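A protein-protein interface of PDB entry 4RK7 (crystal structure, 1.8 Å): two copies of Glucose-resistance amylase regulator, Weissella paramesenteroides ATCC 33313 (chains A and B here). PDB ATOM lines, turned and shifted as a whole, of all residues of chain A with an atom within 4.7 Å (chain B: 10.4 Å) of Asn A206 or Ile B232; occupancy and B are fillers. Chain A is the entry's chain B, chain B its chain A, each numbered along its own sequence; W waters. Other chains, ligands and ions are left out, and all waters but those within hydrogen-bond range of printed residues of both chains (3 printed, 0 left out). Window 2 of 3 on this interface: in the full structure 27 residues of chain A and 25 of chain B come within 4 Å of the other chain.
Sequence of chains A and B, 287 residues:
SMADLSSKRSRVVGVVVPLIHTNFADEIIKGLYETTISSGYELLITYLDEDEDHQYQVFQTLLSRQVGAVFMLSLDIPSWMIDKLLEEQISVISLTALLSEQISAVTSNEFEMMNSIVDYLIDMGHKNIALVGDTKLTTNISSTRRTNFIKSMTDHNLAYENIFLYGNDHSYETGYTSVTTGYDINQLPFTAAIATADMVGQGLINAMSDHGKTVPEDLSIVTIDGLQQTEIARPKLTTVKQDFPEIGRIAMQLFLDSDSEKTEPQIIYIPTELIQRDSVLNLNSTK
Among the printed residues, pairs that only touch across the chains: Asn A206 with Arg B234, Tyr A172 with Arg B234, Tyr A172 with Ile B232, Met A199 with Gln B228, Gln A229 with Ile B232, Met A199 with Ile B232 and Tyr A172 with Gln B228.
Water W1 lies within hydrogen-bond range of the side-chain hydroxyl of Tyr A172 (2.6 Å), the guanidinium group of Arg B234 (2.8 Å) and the side-chain amino group of Lys B236 (3.4 Å). Water W2 lies within hydrogen-bond range of the side-chain amide oxygen (OE1) of Gln B202 (3.0 Å) and the side-chain amide nitrogen (NE2) of Gln A229 (3.1 Å). Water W3 lies within hydrogen-bond range of the backbone NH (N) of Tyr A172 (3.0 Å) and the side-chain amide nitrogen (NE2) of Gln B228 (3.3 Å).
The side-chain amide oxygen (OE1) of Gln B202 is in hydrogen-bond range of the side-chain amide nitrogen (NE2) of Gln B229 (3.1 Å). The backbone carbonyl oxygen (O) of Glu B231 sits at hydrogen-bond distance from the guanidinium group (NH1) of Arg B234 (2.9 Å). The side-chain hydroxyl (OH) of Tyr A172 lies within hydrogen-bond range of the side-chain amide nitrogen (ND2) of Asn A206, at 3.0 Å. The side-chain carboxylate (OD2) of Asp A210 lies within hydrogen-bond range of the side-chain hydroxyl (OH) of Tyr A176. The side-chain amide nitrogen of Gln A202 lies within hydrogen-bond range of the side-chain amide oxygen of Asn A206 (3.2 Å). The side-chain amide nitrogen of Gln A229 lies within hydrogen-bond range of the side-chain amide oxygen of Gln A202 (2.7 Å).
Of the 13 printed residues of chain A, 5 touch a printed residue of chain B. Hydrophobic or aromatic side chains of chain B within 4 Å of the printed part of chain A: Ile B232. Among the printed residues, 10 pairs touch across the chains.
Printed residues of chain B within 4 Å of Asn A206: Ile B232 (2.8 Å) and Arg B234 (3.5 Å). Printed residues of chain A within 4 Å of Ile B232: Tyr A172 (3.5 Å), Met A199 (3.7 Å), Asn A206 (2.8 Å) and Gln A229 (3.7 Å). No residue of chain B comes within 4 Å of Gly A203. No residue of chain B comes within 4 Å of Ile A205. Asp A210 touches one residue of chain B. Of the printed residues of chain B, Met A199 touches Gln B228 and Ile B232. Of the printed residues of chain A, Gln B228 touches Tyr A172 (3.9 Å) and Met A199 (3.6 Å). Met B199 touches none of the printed residues of chain A. Met A208 touches none of the printed residues of chain B.
The side-chain amide oxygen of Gln A229 is in hydrogen-bond range of the side-chain amide nitrogen of Gln B229, at 3.2 Å. O of Ile B232 lies within hydrogen-bond range of ND2 of Asn A206, at 2.8 Å. NH2 of Arg B234 lies within salt-bridge range of OD2 of Asp A210 (2.8 Å).
Gln B229 touches its own counterpart, Gln A229. Positions printed for both chains: 199, 202, 205, 206 and 229. Of the 10 pairs that touch across the chains among the printed residues, 1 has its exchanged pair printed and touching as well.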
ATOM      1  N   TYR A 172       6.833  -3.609 -22.300  1.00  0.00           N
ATOM      2  CA  TYR A 172       6.919  -5.043 -22.420  1.00  0.00           C
ATOM      3  C   TYR A 172       7.775  -5.491 -23.587  1.00  0.00           C
ATOM      4  O   TYR A 172       8.615  -6.357 -23.441  1.00  0.00           O
ATOM      5  CB  TYR A 172       5.508  -5.620 -22.580  1.00  0.00           C
ATOM      6  CG  TYR A 172       5.453  -7.103 -22.755  1.00  0.00           C
ATOM      7  CD1 TYR A 172       5.439  -7.969 -21.650  1.00  0.00           C
ATOM      8  CD2 TYR A 172       5.361  -7.667 -24.024  1.00  0.00           C
ATOM      9  CE1 TYR A 172       5.343  -9.334 -21.830  1.00  0.00           C
ATOM     10  CE2 TYR A 172       5.273  -9.036 -24.204  1.00  0.00           C
ATOM     11  CZ  TYR A 172       5.269  -9.864 -23.109  1.00  0.00           C
ATOM     12  OH  TYR A 172       5.166 -11.196 -23.317  1.00  0.00           O
ATOM     13  N   TYR A 176      11.075  -7.972 -23.763  1.00  0.00           N
ATOM     14  CA  TYR A 176      11.010  -9.203 -24.528  1.00  0.00           C
ATOM     15  C   TYR A 176      12.147  -9.233 -25.568  1.00  0.00           C
ATOM     16  O   TYR A 176      12.801 -10.258 -25.721  1.00  0.00           O
ATOM     17  CB  TYR A 176       9.638  -9.361 -25.221  1.00  0.00           C
ATOM     18  CG  TYR A 176       9.345 -10.792 -25.572  1.00  0.00           C
ATOM     19  CD1 TYR A 176       9.927 -11.381 -26.686  1.00  0.00           C
ATOM     20  CD2 TYR A 176       8.486 -11.573 -24.790  1.00  0.00           C
ATOM     21  CE1 TYR A 176       9.700 -12.712 -27.000  1.00  0.00           C
ATOM     22  CE2 TYR A 176       8.241 -12.905 -25.099  1.00  0.00           C
ATOM     23  CZ  TYR A 176       8.844 -13.467 -26.218  1.00  0.00           C
ATOM     24  OH  TYR A 176       8.625 -14.795 -26.512  1.00  0.00           O
ATOM     25  N   MET A 199       6.657  -3.653 -16.502  1.00  0.00           N
ATOM     26  CA  MET A 199       6.316  -4.363 -17.742  1.00  0.00           C
ATOM     27  C   MET A 199       7.554  -4.856 -18.467  1.00  0.00           C
ATOM     28  O   MET A 199       7.512  -5.890 -19.124  1.00  0.00           O
ATOM     29  CB  MET A 199       5.466  -3.533 -18.702  1.00  0.00           C
ATOM     30  CG  MET A 199       4.020  -3.482 -18.269  1.00  0.00           C
ATOM     31  SD  MET A 199       3.300  -5.283 -18.643  1.00  0.00           S
ATOM     32  CE  MET A 199       1.483  -4.646 -18.223  1.00  0.00           C
ATOM     33  N   GLN A 202       8.232  -8.104 -16.919  1.00  0.00           N
ATOM     34  CA  GLN A 202       7.318  -9.128 -17.398  1.00  0.00           C
ATOM     35  C   GLN A 202       7.717  -9.625 -18.804  1.00  0.00           C
ATOM     36  O   GLN A 202       7.656 -10.827 -19.084  1.00  0.00           O
ATOM     37  CB  GLN A 202       5.869  -8.628 -17.395  1.00  0.00           C
ATOM     38  CG  GLN A 202       4.882  -9.735 -17.684  1.00  0.00           C
ATOM     39  CD  GLN A 202       4.961 -10.839 -16.630  1.00  0.00           C
ATOM     40  OE1 GLN A 202       4.728 -10.577 -15.465  1.00  0.00           O
ATOM     41  NE2 GLN A 202       5.292 -12.058 -17.035  1.00  0.00           N
ATOM     42  N   GLY A 203       8.135  -8.705 -19.664  1.00  0.00           N
ATOM     43  CA  GLY A 203       8.677  -9.078 -20.979  1.00  0.00           C
ATOM     44  C   GLY A 203       9.883  -9.995 -20.881  1.00  0.00           C
ATOM     45  O   GLY A 203       9.990 -10.969 -21.622  1.00  0.00           O
ATOM     46  N   LEU A 204      10.794  -9.686 -19.957  1.00  0.00           N
ATOM     47  CA  LEU A 204      11.951 -10.548 -19.720  1.00  0.00           C
ATOM     48  C   LEU A 204      11.530 -11.944 -19.249  1.00  0.00           C
ATOM     49  O   LEU A 204      12.022 -12.957 -19.765  1.00  0.00           O
ATOM     50  CB  LEU A 204      12.905  -9.903 -18.700  1.00  0.00           C
ATOM     51  CG  LEU A 204      13.762  -8.745 -19.232  1.00  0.00           C
ATOM     52  CD1 LEU A 204      14.290  -7.899 -18.066  1.00  0.00           C
ATOM     53  CD2 LEU A 204      14.899  -9.257 -20.091  1.00  0.00           C
ATOM     54  N   ILE A 205      10.614 -12.006 -18.271  1.00  0.00           N
ATOM     55  CA  ILE A 205      10.117 -13.288 -17.784  1.00  0.00           C
ATOM     56  C   ILE A 205       9.533 -14.132 -18.912  1.00  0.00           C
ATOM     57  O   ILE A 205       9.852 -15.325 -19.052  1.00  0.00           O
ATOM     58  CB  ILE A 205       9.069 -13.123 -16.651  1.00  0.00           C
ATOM     59  CG1 ILE A 205       9.774 -12.704 -15.359  1.00  0.00           C
ATOM     60  CG2 ILE A 205       8.321 -14.431 -16.424  1.00  0.00           C
ATOM     61  CD1 ILE A 205       8.823 -12.461 -14.210  1.00  0.00           C
ATOM     62  N   ASN A 206       8.675 -13.518 -19.723  1.00  0.00           N
ATOM     63  CA  ASN A 206       8.019 -14.256 -20.790  1.00  0.00           C
ATOM     64  C   ASN A 206       8.982 -14.697 -21.888  1.00  0.00           C
ATOM     65  O   ASN A 206       8.847 -15.807 -22.413  1.00  0.00           O
ATOM     66  CB  ASN A 206       6.842 -13.448 -21.364  1.00  0.00           C
ATOM     67  CG  ASN A 206       5.620 -13.484 -20.471  1.00  0.00           C
ATOM     68  OD1 ASN A 206       5.627 -14.129 -19.414  1.00  0.00           O
ATOM     69  ND2 ASN A 206       4.555 -12.820 -20.898  1.00  0.00           N
ATOM     70  N   ALA A 207       9.949 -13.855 -22.242  1.00  0.00           N
ATOM     71  CA  ALA A 207      10.943 -14.242 -23.269  1.00  0.00           C
ATOM     72  C   ALA A 207      11.758 -15.451 -22.790  1.00  0.00           C
ATOM     73  O   ALA A 207      12.002 -16.410 -23.534  1.00  0.00           O
ATOM     74  CB  ALA A 207      11.865 -13.059 -23.603  1.00  0.00           C
ATOM     75  N   MET A 208      12.141 -15.433 -21.529  1.00  0.00           N
ATOM     76  CA  MET A 208      12.877 -16.555 -20.957  1.00  0.00           C
ATOM     77  C   MET A 208      12.039 -17.805 -20.960  1.00  0.00           C
ATOM     78  O   MET A 208      12.470 -18.862 -21.458  1.00  0.00           O
ATOM     79  CB  MET A 208      13.386 -16.215 -19.546  1.00  0.00           C
ATOM     80  CG  MET A 208      14.373 -15.071 -19.406  1.00  0.00           C
ATOM     81  SD  MET A 208      15.966 -15.221 -20.577  1.00  0.00           S
ATOM     82  CE  MET A 208      16.901 -16.558 -19.496  1.00  0.00           C
ATOM     83  N   SER A 209      10.826 -17.714 -20.428  1.00  0.00           N
ATOM     84  CA  SER A 209       9.935 -18.868 -20.368  1.00  0.00           C
ATOM     85  C   SER A 209       9.566 -19.395 -21.756  1.00  0.00           C
ATOM     86  O   SER A 209       9.544 -20.617 -21.980  1.00  0.00           O
ATOM     87  CB  SER A 209       8.663 -18.543 -19.575  1.00  0.00           C
ATOM     88  OG  SER A 209       7.976 -19.739 -19.257  1.00  0.00           O
ATOM     89  N   ASP A 210       9.283 -18.493 -22.686  1.00  0.00           N
ATOM     90  CA  ASP A 210       8.920 -18.906 -24.030  1.00  0.00           C
ATOM     91  C   ASP A 210      10.036 -19.678 -24.752  1.00  0.00           C
ATOM     92  O   ASP A 210       9.752 -20.406 -25.706  1.00  0.00           O
ATOM     93  CB  ASP A 210       8.516 -17.713 -24.884  1.00  0.00           C
ATOM     94  CG  ASP A 210       7.160 -17.092 -24.460  1.00  0.00           C
ATOM     95  OD1 ASP A 210       6.432 -17.667 -23.624  1.00  0.00           O
ATOM     96  OD2 ASP A 210       6.862 -15.990 -24.971  1.00  0.00           O
ATOM     97  N   GLN A 229       1.704  -5.662 -11.531  1.00  0.00           N
ATOM     98  CA  GLN A 229       2.289  -6.676 -12.389  1.00  0.00           C
ATOM     99  C   GLN A 229       3.400  -7.445 -11.684  1.00  0.00           C
ATOM    100  O   GLN A 229       3.646  -8.624 -11.989  1.00  0.00           O
ATOM    101  CB  GLN A 229       2.804  -6.050 -13.691  1.00  0.00           C
ATOM    102  CG  GLN A 229       3.241  -7.074 -14.718  1.00  0.00           C
ATOM    103  CD  GLN A 229       2.108  -7.989 -15.165  1.00  0.00           C
ATOM    104  OE1 GLN A 229       1.012  -7.526 -15.413  1.00  0.00           O
ATOM    105  NE2 GLN A 229       2.386  -9.290 -15.284  1.00  0.00           N
ATOM    106  N   ASN B  23      -8.375  -1.076 -17.309  1.00  0.00           N
ATOM    107  CA  ASN B  23      -7.756  -0.272 -18.377  1.00  0.00           C
ATOM    108  C   ASN B  23      -8.619  -0.043 -19.627  1.00  0.00           C
ATOM    109  O   ASN B  23      -8.141   0.549 -20.606  1.00  0.00           O
ATOM    110  CB  ASN B  23      -6.397  -0.863 -18.792  1.00  0.00           C
ATOM    111  CG  ASN B  23      -5.247  -0.345 -17.940  1.00  0.00           C
ATOM    112  OD1 ASN B  23      -5.206   0.835 -17.569  1.00  0.00           O
ATOM    113  ND2 ASN B  23      -4.297  -1.222 -17.638  1.00  0.00           N
ATOM    114  N   ASP B 198     -10.326  -9.270 -18.209  1.00  0.00           N
ATOM    115  CA  ASP B 198      -9.050  -9.944 -18.436  1.00  0.00           C
ATOM    116  C   ASP B 198      -8.302 -10.310 -17.121  1.00  0.00           C
ATOM    117  O   ASP B 198      -7.756 -11.410 -16.986  1.00  0.00           O
ATOM    118  CB  ASP B 198      -8.132  -9.080 -19.296  1.00  0.00           C
ATOM    119  CG  ASP B 198      -8.742  -8.731 -20.667  1.00  0.00           C
ATOM    120  OD1 ASP B 198      -9.538  -9.536 -21.238  1.00  0.00           O
ATOM    121  OD2 ASP B 198      -8.357  -7.649 -21.151  1.00  0.00           O
ATOM    122  N   MET B 199      -8.290  -9.384 -16.164  1.00  0.00           N
ATOM    123  CA  MET B 199      -7.546  -9.590 -14.906  1.00  0.00           C
ATOM    124  C   MET B 199      -8.159 -10.743 -14.125  1.00  0.00           C
ATOM    125  O   MET B 199      -7.454 -11.463 -13.439  1.00  0.00           O
ATOM    126  CB  MET B 199      -7.518  -8.334 -14.029  1.00  0.00           C
ATOM    127  CG  MET B 199      -6.381  -7.421 -14.417  1.00  0.00           C
ATOM    128  SD  MET B 199      -4.715  -8.312 -13.878  1.00  0.00           S
ATOM    129  CE  MET B 199      -3.646  -6.739 -14.386  1.00  0.00           C
ATOM    130  N   GLY B 201      -9.325 -13.414 -15.493  1.00  0.00           N
ATOM    131  CA  GLY B 201      -8.658 -14.541 -16.121  1.00  0.00           C
ATOM    132  C   GLY B 201      -7.224 -14.762 -15.657  1.00  0.00           C
ATOM    133  O   GLY B 201      -6.790 -15.903 -15.447  1.00  0.00           O
ATOM    134  N   GLN B 202      -6.493 -13.672 -15.459  1.00  0.00           N
ATOM    135  CA  GLN B 202      -5.133 -13.767 -14.950  1.00  0.00           C
ATOM    136  C   GLN B 202      -5.115 -14.330 -13.518  1.00  0.00           C
ATOM    137  O   GLN B 202      -4.203 -15.103 -13.155  1.00  0.00           O
ATOM    138  CB  GLN B 202      -4.480 -12.408 -15.002  1.00  0.00           C
ATOM    139  CG  GLN B 202      -3.073 -12.391 -14.502  1.00  0.00           C
ATOM    140  CD  GLN B 202      -2.122 -13.126 -15.414  1.00  0.00           C
ATOM    141  OE1 GLN B 202      -1.671 -12.568 -16.416  1.00  0.00           O
ATOM    142  NE2 GLN B 202      -1.776 -14.365 -15.056  1.00  0.00           N
ATOM    143  N   ILE B 205      -5.658 -18.094 -13.810  1.00  0.00           N
ATOM    144  CA  ILE B 205      -4.428 -18.750 -14.229  1.00  0.00           C
ATOM    145  C   ILE B 205      -3.466 -18.924 -13.052  1.00  0.00           C
ATOM    146  O   ILE B 205      -2.912 -20.018 -12.840  1.00  0.00           O
ATOM    147  CB  ILE B 205      -3.736 -17.939 -15.349  1.00  0.00           C
ATOM    148  CG1 ILE B 205      -4.478 -18.177 -16.670  1.00  0.00           C
ATOM    149  CG2 ILE B 205      -2.283 -18.366 -15.505  1.00  0.00           C
ATOM    150  CD1 ILE B 205      -3.893 -17.377 -17.825  1.00  0.00           C
ATOM    151  N   ASN B 206      -3.270 -17.862 -12.280  1.00  0.00           N
ATOM    152  CA  ASN B 206      -2.278 -17.930 -11.192  1.00  0.00           C
ATOM    153  C   ASN B 206      -2.737 -18.848 -10.071  1.00  0.00           C
ATOM    154  O   ASN B 206      -1.905 -19.556  -9.494  1.00  0.00           O
ATOM    155  CB  ASN B 206      -1.893 -16.542 -10.662  1.00  0.00           C
ATOM    156  CG  ASN B 206      -0.936 -15.813 -11.580  1.00  0.00           C
ATOM    157  OD1 ASN B 206      -0.460 -16.378 -12.548  1.00  0.00           O
ATOM    158  ND2 ASN B 206      -0.639 -14.565 -11.274  1.00  0.00           N
ATOM    159  N   THR B 223     -11.866 -14.830 -21.553  1.00  0.00           N
ATOM    160  CA  THR B 223     -12.092 -13.530 -20.909  1.00  0.00           C
ATOM    161  C   THR B 223     -12.840 -12.559 -21.811  1.00  0.00           C
ATOM    162  O   THR B 223     -12.895 -12.737 -23.023  1.00  0.00           O
ATOM    163  CB  THR B 223     -10.818 -12.806 -20.450  1.00  0.00           C
ATOM    164  OG1 THR B 223     -10.168 -12.179 -21.561  1.00  0.00           O
ATOM    165  CG2 THR B 223      -9.850 -13.732 -19.748  1.00  0.00           C
ATOM    166  N   GLY B 226     -10.103  -8.336 -23.955  1.00  0.00           N
ATOM    167  CA  GLY B 226      -9.033  -8.578 -24.919  1.00  0.00           C
ATOM    168  C   GLY B 226      -7.934  -7.546 -24.918  1.00  0.00           C
ATOM    169  O   GLY B 226      -7.316  -7.298 -25.951  1.00  0.00           O
ATOM    170  N   LEU B 227      -7.678  -6.954 -23.762  1.00  0.00           N
ATOM    171  CA  LEU B 227      -6.605  -5.979 -23.606  1.00  0.00           C
ATOM    172  C   LEU B 227      -5.261  -6.693 -23.325  1.00  0.00           C
ATOM    173  O   LEU B 227      -5.189  -7.928 -23.405  1.00  0.00           O
ATOM    174  CB  LEU B 227      -6.985  -4.965 -22.554  1.00  0.00           C
ATOM    175  CG  LEU B 227      -8.161  -4.072 -23.001  1.00  0.00           C
ATOM    176  CD1 LEU B 227      -8.641  -3.227 -21.846  1.00  0.00           C
ATOM    177  CD2 LEU B 227      -7.784  -3.192 -24.175  1.00  0.00           C
ATOM    178  N   GLN B 228      -4.215  -5.912 -23.024  1.00  0.00           N
ATOM    179  CA  GLN B 228      -2.836  -6.442 -23.051  1.00  0.00           C
ATOM    180  C   GLN B 228      -2.593  -7.595 -22.085  1.00  0.00           C
ATOM    181  O   GLN B 228      -1.773  -8.465 -22.361  1.00  0.00           O
ATOM    182  CB  GLN B 228      -1.852  -5.318 -22.753  1.00  0.00           C
ATOM    183  CG  GLN B 228      -0.395  -5.753 -22.704  1.00  0.00           C
ATOM    184  CD  GLN B 228       0.541  -4.617 -22.324  1.00  0.00           C
ATOM    185  OE1 GLN B 228       0.197  -3.753 -21.511  1.00  0.00           O
ATOM    186  NE2 GLN B 228       1.736  -4.619 -22.904  1.00  0.00           N
ATOM    187  N   GLN B 229      -3.299  -7.641 -20.966  1.00  0.00           N
ATOM    188  CA  GLN B 229      -3.117  -8.798 -20.047  1.00  0.00           C
ATOM    189  C   GLN B 229      -3.345 -10.151 -20.720  1.00  0.00           C
ATOM    190  O   GLN B 229      -2.707 -11.146 -20.346  1.00  0.00           O
ATOM    191  CB  GLN B 229      -3.991  -8.679 -18.804  1.00  0.00           C
ATOM    192  CG  GLN B 229      -3.422  -9.387 -17.596  1.00  0.00           C
ATOM    193  CD  GLN B 229      -2.133  -8.713 -17.097  1.00  0.00           C
ATOM    194  OE1 GLN B 229      -2.009  -7.477 -17.108  1.00  0.00           O
ATOM    195  NE2 GLN B 229      -1.195  -9.508 -16.663  1.00  0.00           N
ATOM    196  N   THR B 230      -4.243 -10.215 -21.715  1.00  0.00           N
ATOM    197  CA  THR B 230      -4.511 -11.470 -22.400  1.00  0.00           C
ATOM    198  C   THR B 230      -3.333 -11.960 -23.222  1.00  0.00           C
ATOM    199  O   THR B 230      -3.212 -13.155 -23.443  1.00  0.00           O
ATOM    200  CB  THR B 230      -5.774 -11.428 -23.286  1.00  0.00           C
ATOM    201  OG1 THR B 230      -5.571 -10.505 -24.365  1.00  0.00           O
ATOM    202  CG2 THR B 230      -6.979 -11.025 -22.460  1.00  0.00           C
ATOM    203  N   GLU B 231      -2.463 -11.032 -23.631  1.00  0.00           N
ATOM    204  CA  GLU B 231      -1.277 -11.349 -24.436  1.00  0.00           C
ATOM    205  C   GLU B 231      -0.047 -11.656 -23.572  1.00  0.00           C
ATOM    206  O   GLU B 231       0.853 -12.352 -24.013  1.00  0.00           O
ATOM    207  CB  GLU B 231      -0.911 -10.167 -25.331  1.00  0.00           C
ATOM    208  CG  GLU B 231      -1.980  -9.715 -26.334  1.00  0.00           C
ATOM    209  CD  GLU B 231      -1.842  -8.237 -26.722  1.00  0.00           C
ATOM    210  OE1 GLU B 231      -0.752  -7.642 -26.543  1.00  0.00           O
ATOM    211  OE2 GLU B 231      -2.834  -7.646 -27.200  1.00  0.00           O
ATOM    212  N   ILE B 232      -0.021 -11.103 -22.367  1.00  0.00           N
ATOM    213  CA  ILE B 232       1.141 -11.317 -21.495  1.00  0.00           C
ATOM    214  C   ILE B 232       0.915 -12.478 -20.533  1.00  0.00           C
ATOM    215  O   ILE B 232       1.868 -13.022 -20.003  1.00  0.00           O
ATOM    216  CB  ILE B 232       1.615 -10.023 -20.794  1.00  0.00           C
ATOM    217  CG1 ILE B 232       0.638  -9.568 -19.709  1.00  0.00           C
ATOM    218  CG2 ILE B 232       1.846  -8.927 -21.817  1.00  0.00           C
ATOM    219  CD1 ILE B 232       1.032  -8.255 -19.065  1.00  0.00           C
ATOM    220  N   ALA B 233      -0.333 -12.902 -20.351  1.00  0.00           N
ATOM    221  CA  ALA B 233      -0.620 -14.131 -19.628  1.00  0.00           C
ATOM    222  C   ALA B 233       0.041 -15.324 -20.287  1.00  0.00           C
ATOM    223  O   ALA B 233       0.266 -15.353 -21.497  1.00  0.00           O
ATOM    224  CB  ALA B 233      -2.130 -14.370 -19.570  1.00  0.00           C
ATOM    225  N   ARG B 234       0.325 -16.330 -19.484  1.00  0.00           N
ATOM    226  CA  ARG B 234       0.832 -17.606 -19.990  1.00  0.00           C
ATOM    227  C   ARG B 234       0.080 -18.710 -19.273  1.00  0.00           C
ATOM    228  O   ARG B 234       0.257 -18.876 -18.048  1.00  0.00           O
ATOM    229  CB  ARG B 234       2.348 -17.733 -19.751  1.00  0.00           C
ATOM    230  CG  ARG B 234       3.216 -16.807 -20.593  1.00  0.00           C
ATOM    231  CD  ARG B 234       3.185 -17.209 -22.077  1.00  0.00           C
ATOM    232  NE  ARG B 234       4.035 -16.375 -22.934  1.00  0.00           N
ATOM    233  CZ  ARG B 234       3.710 -15.181 -23.430  1.00  0.00           C
ATOM    234  NH1 ARG B 234       2.540 -14.599 -23.150  1.00  0.00           N
ATOM    235  NH2 ARG B 234       4.579 -14.549 -24.210  1.00  0.00           N
ATOM    236  N   PRO B 235      -0.755 -19.484 -19.972  1.00  0.00           N
ATOM    237  CA  PRO B 235      -1.016 -19.417 -21.417  1.00  0.00           C
ATOM    238  C   PRO B 235      -1.692 -18.127 -21.846  1.00  0.00           C
ATOM    239  O   PRO B 235      -2.440 -17.516 -21.063  1.00  0.00           O
ATOM    240  CB  PRO B 235      -2.012 -20.563 -21.629  1.00  0.00           C
ATOM    241  CG  PRO B 235      -2.754 -20.641 -20.328  1.00  0.00           C
ATOM    242  CD  PRO B 235      -1.697 -20.390 -19.288  1.00  0.00           C
ATOM    243  N   LYS B 236      -1.446 -17.696 -23.083  1.00  0.00           N
ATOM    244  CA  LYS B 236      -2.153 -16.540 -23.622  1.00  0.00           C
ATOM    245  C   LYS B 236      -3.663 -16.834 -23.581  1.00  0.00           C
ATOM    246  O   LYS B 236      -4.083 -17.953 -23.869  1.00  0.00           O
ATOM    247  CB  LYS B 236      -1.708 -16.244 -25.060  1.00  0.00           C
ATOM    248  CG  LYS B 236      -0.285 -15.711 -25.205  1.00  0.00           C
ATOM    249  CD  LYS B 236       0.172 -15.670 -26.663  1.00  0.00           C
ATOM    250  CE  LYS B 236       1.479 -14.896 -26.841  1.00  0.00           C
ATOM    251  NZ  LYS B 236       1.335 -13.409 -26.981  1.00  0.00           N
ATOM    252  N   LEU B 237      -4.454 -15.828 -23.214  1.00  0.00           N
ATOM    253  CA  LEU B 237      -5.891 -15.987 -22.980  1.00  0.00           C
ATOM    254  C   LEU B 237      -6.741 -15.766 -24.219  1.00  0.00           C
ATOM    255  O   LEU B 237      -6.648 -14.730 -24.907  1.00  0.00           O
ATOM    256  CB  LEU B 237      -6.364 -15.038 -21.885  1.00  0.00           C
ATOM    257  CG  LEU B 237      -5.958 -15.433 -20.466  1.00  0.00           C
ATOM    258  CD1 LEU B 237      -5.926 -14.193 -19.584  1.00  0.00           C
ATOM    259  CD2 LEU B 237      -6.903 -16.503 -19.884  1.00  0.00           C
ATOM    260  N   THR B 238      -7.560 -16.760 -24.472  1.00  0.00           N
ATOM    261  CA  THR B 238      -8.676 -16.656 -25.404  1.00  0.00           C
ATOM    262  C   THR B 238      -9.618 -15.601 -24.844  1.00  0.00           C
ATOM    263  O   THR B 238      -9.884 -15.542 -23.621  1.00  0.00           O
ATOM    264  CB  THR B 238      -9.320 -18.031 -25.579  1.00  0.00           C
ATOM    265  OG1 THR B 238      -8.356 -18.907 -26.191  1.00  0.00           O
ATOM    266  CG2 THR B 238     -10.559 -17.983 -26.450  1.00  0.00           C
ATOM    267  N   THR B 239     -10.109 -14.736 -25.724  1.00  0.00           N
ATOM    268  CA  THR B 239     -10.777 -13.527 -25.272  1.00  0.00           C
ATOM    269  C   THR B 239     -11.778 -12.996 -26.305  1.00  0.00           C
ATOM    270  O   THR B 239     -11.583 -13.162 -27.505  1.00  0.00           O
ATOM    271  CB  THR B 239      -9.728 -12.449 -24.919  1.00  0.00           C
ATOM    272  OG1 THR B 239     -10.343 -11.372 -24.218  1.00  0.00           O
ATOM    273  CG2 THR B 239      -8.961 -11.914 -26.116  1.00  0.00           C
ATOM    274  N   ARG B 277      -6.769 -18.152 -28.450  1.00  0.00           N
ATOM    275  CA  ARG B 277      -5.345 -18.273 -28.107  1.00  0.00           C
ATOM    276  C   ARG B 277      -5.109 -19.643 -27.468  1.00  0.00           C
ATOM    277  O   ARG B 277      -5.398 -20.652 -28.092  1.00  0.00           O
ATOM    278  CB  ARG B 277      -4.883 -17.082 -27.259  1.00  0.00           C
ATOM    279  CG  ARG B 277      -5.147 -15.730 -27.917  1.00  0.00           C
ATOM    280  CD  ARG B 277      -4.133 -14.682 -27.517  1.00  0.00           C
ATOM    281  NE  ARG B 277      -4.283 -13.380 -28.194  1.00  0.00           N
ATOM    282  CZ  ARG B 277      -4.883 -12.320 -27.667  1.00  0.00           C
ATOM    283  NH1 ARG B 277      -5.479 -12.390 -26.488  1.00  0.00           N
ATOM    284  NH2 ARG B 277      -4.913 -11.179 -28.336  1.00  0.00           N
ATOM    285  N   ASP B 278      -4.605 -19.708 -26.241  1.00  0.00           N
ATOM    286  CA  ASP B 278      -4.063 -20.959 -25.703  1.00  0.00           C
ATOM    287  C   ASP B 278      -4.732 -21.462 -24.434  1.00  0.00           C
ATOM    288  O   ASP B 278      -4.264 -22.415 -23.829  1.00  0.00           O
ATOM    289  CB  ASP B 278      -2.546 -20.780 -25.479  1.00  0.00           C
ATOM    290  CG  ASP B 278      -1.809 -20.474 -26.777  1.00  0.00           C
ATOM    291  OD1 ASP B 278      -2.156 -21.081 -27.804  1.00  0.00           O
ATOM    292  OD2 ASP B 278      -0.906 -19.617 -26.776  1.00  0.00           O
HETATM  293  O   HOH W   1       4.121 -12.061 -25.519  1.00  0.00           O
HETATM  294  O   HOH W   2       1.261 -11.968 -16.216  1.00  0.00           O
HETATM  295  O   HOH W   3       4.067  -2.356 -22.341  1.00  0.00           O
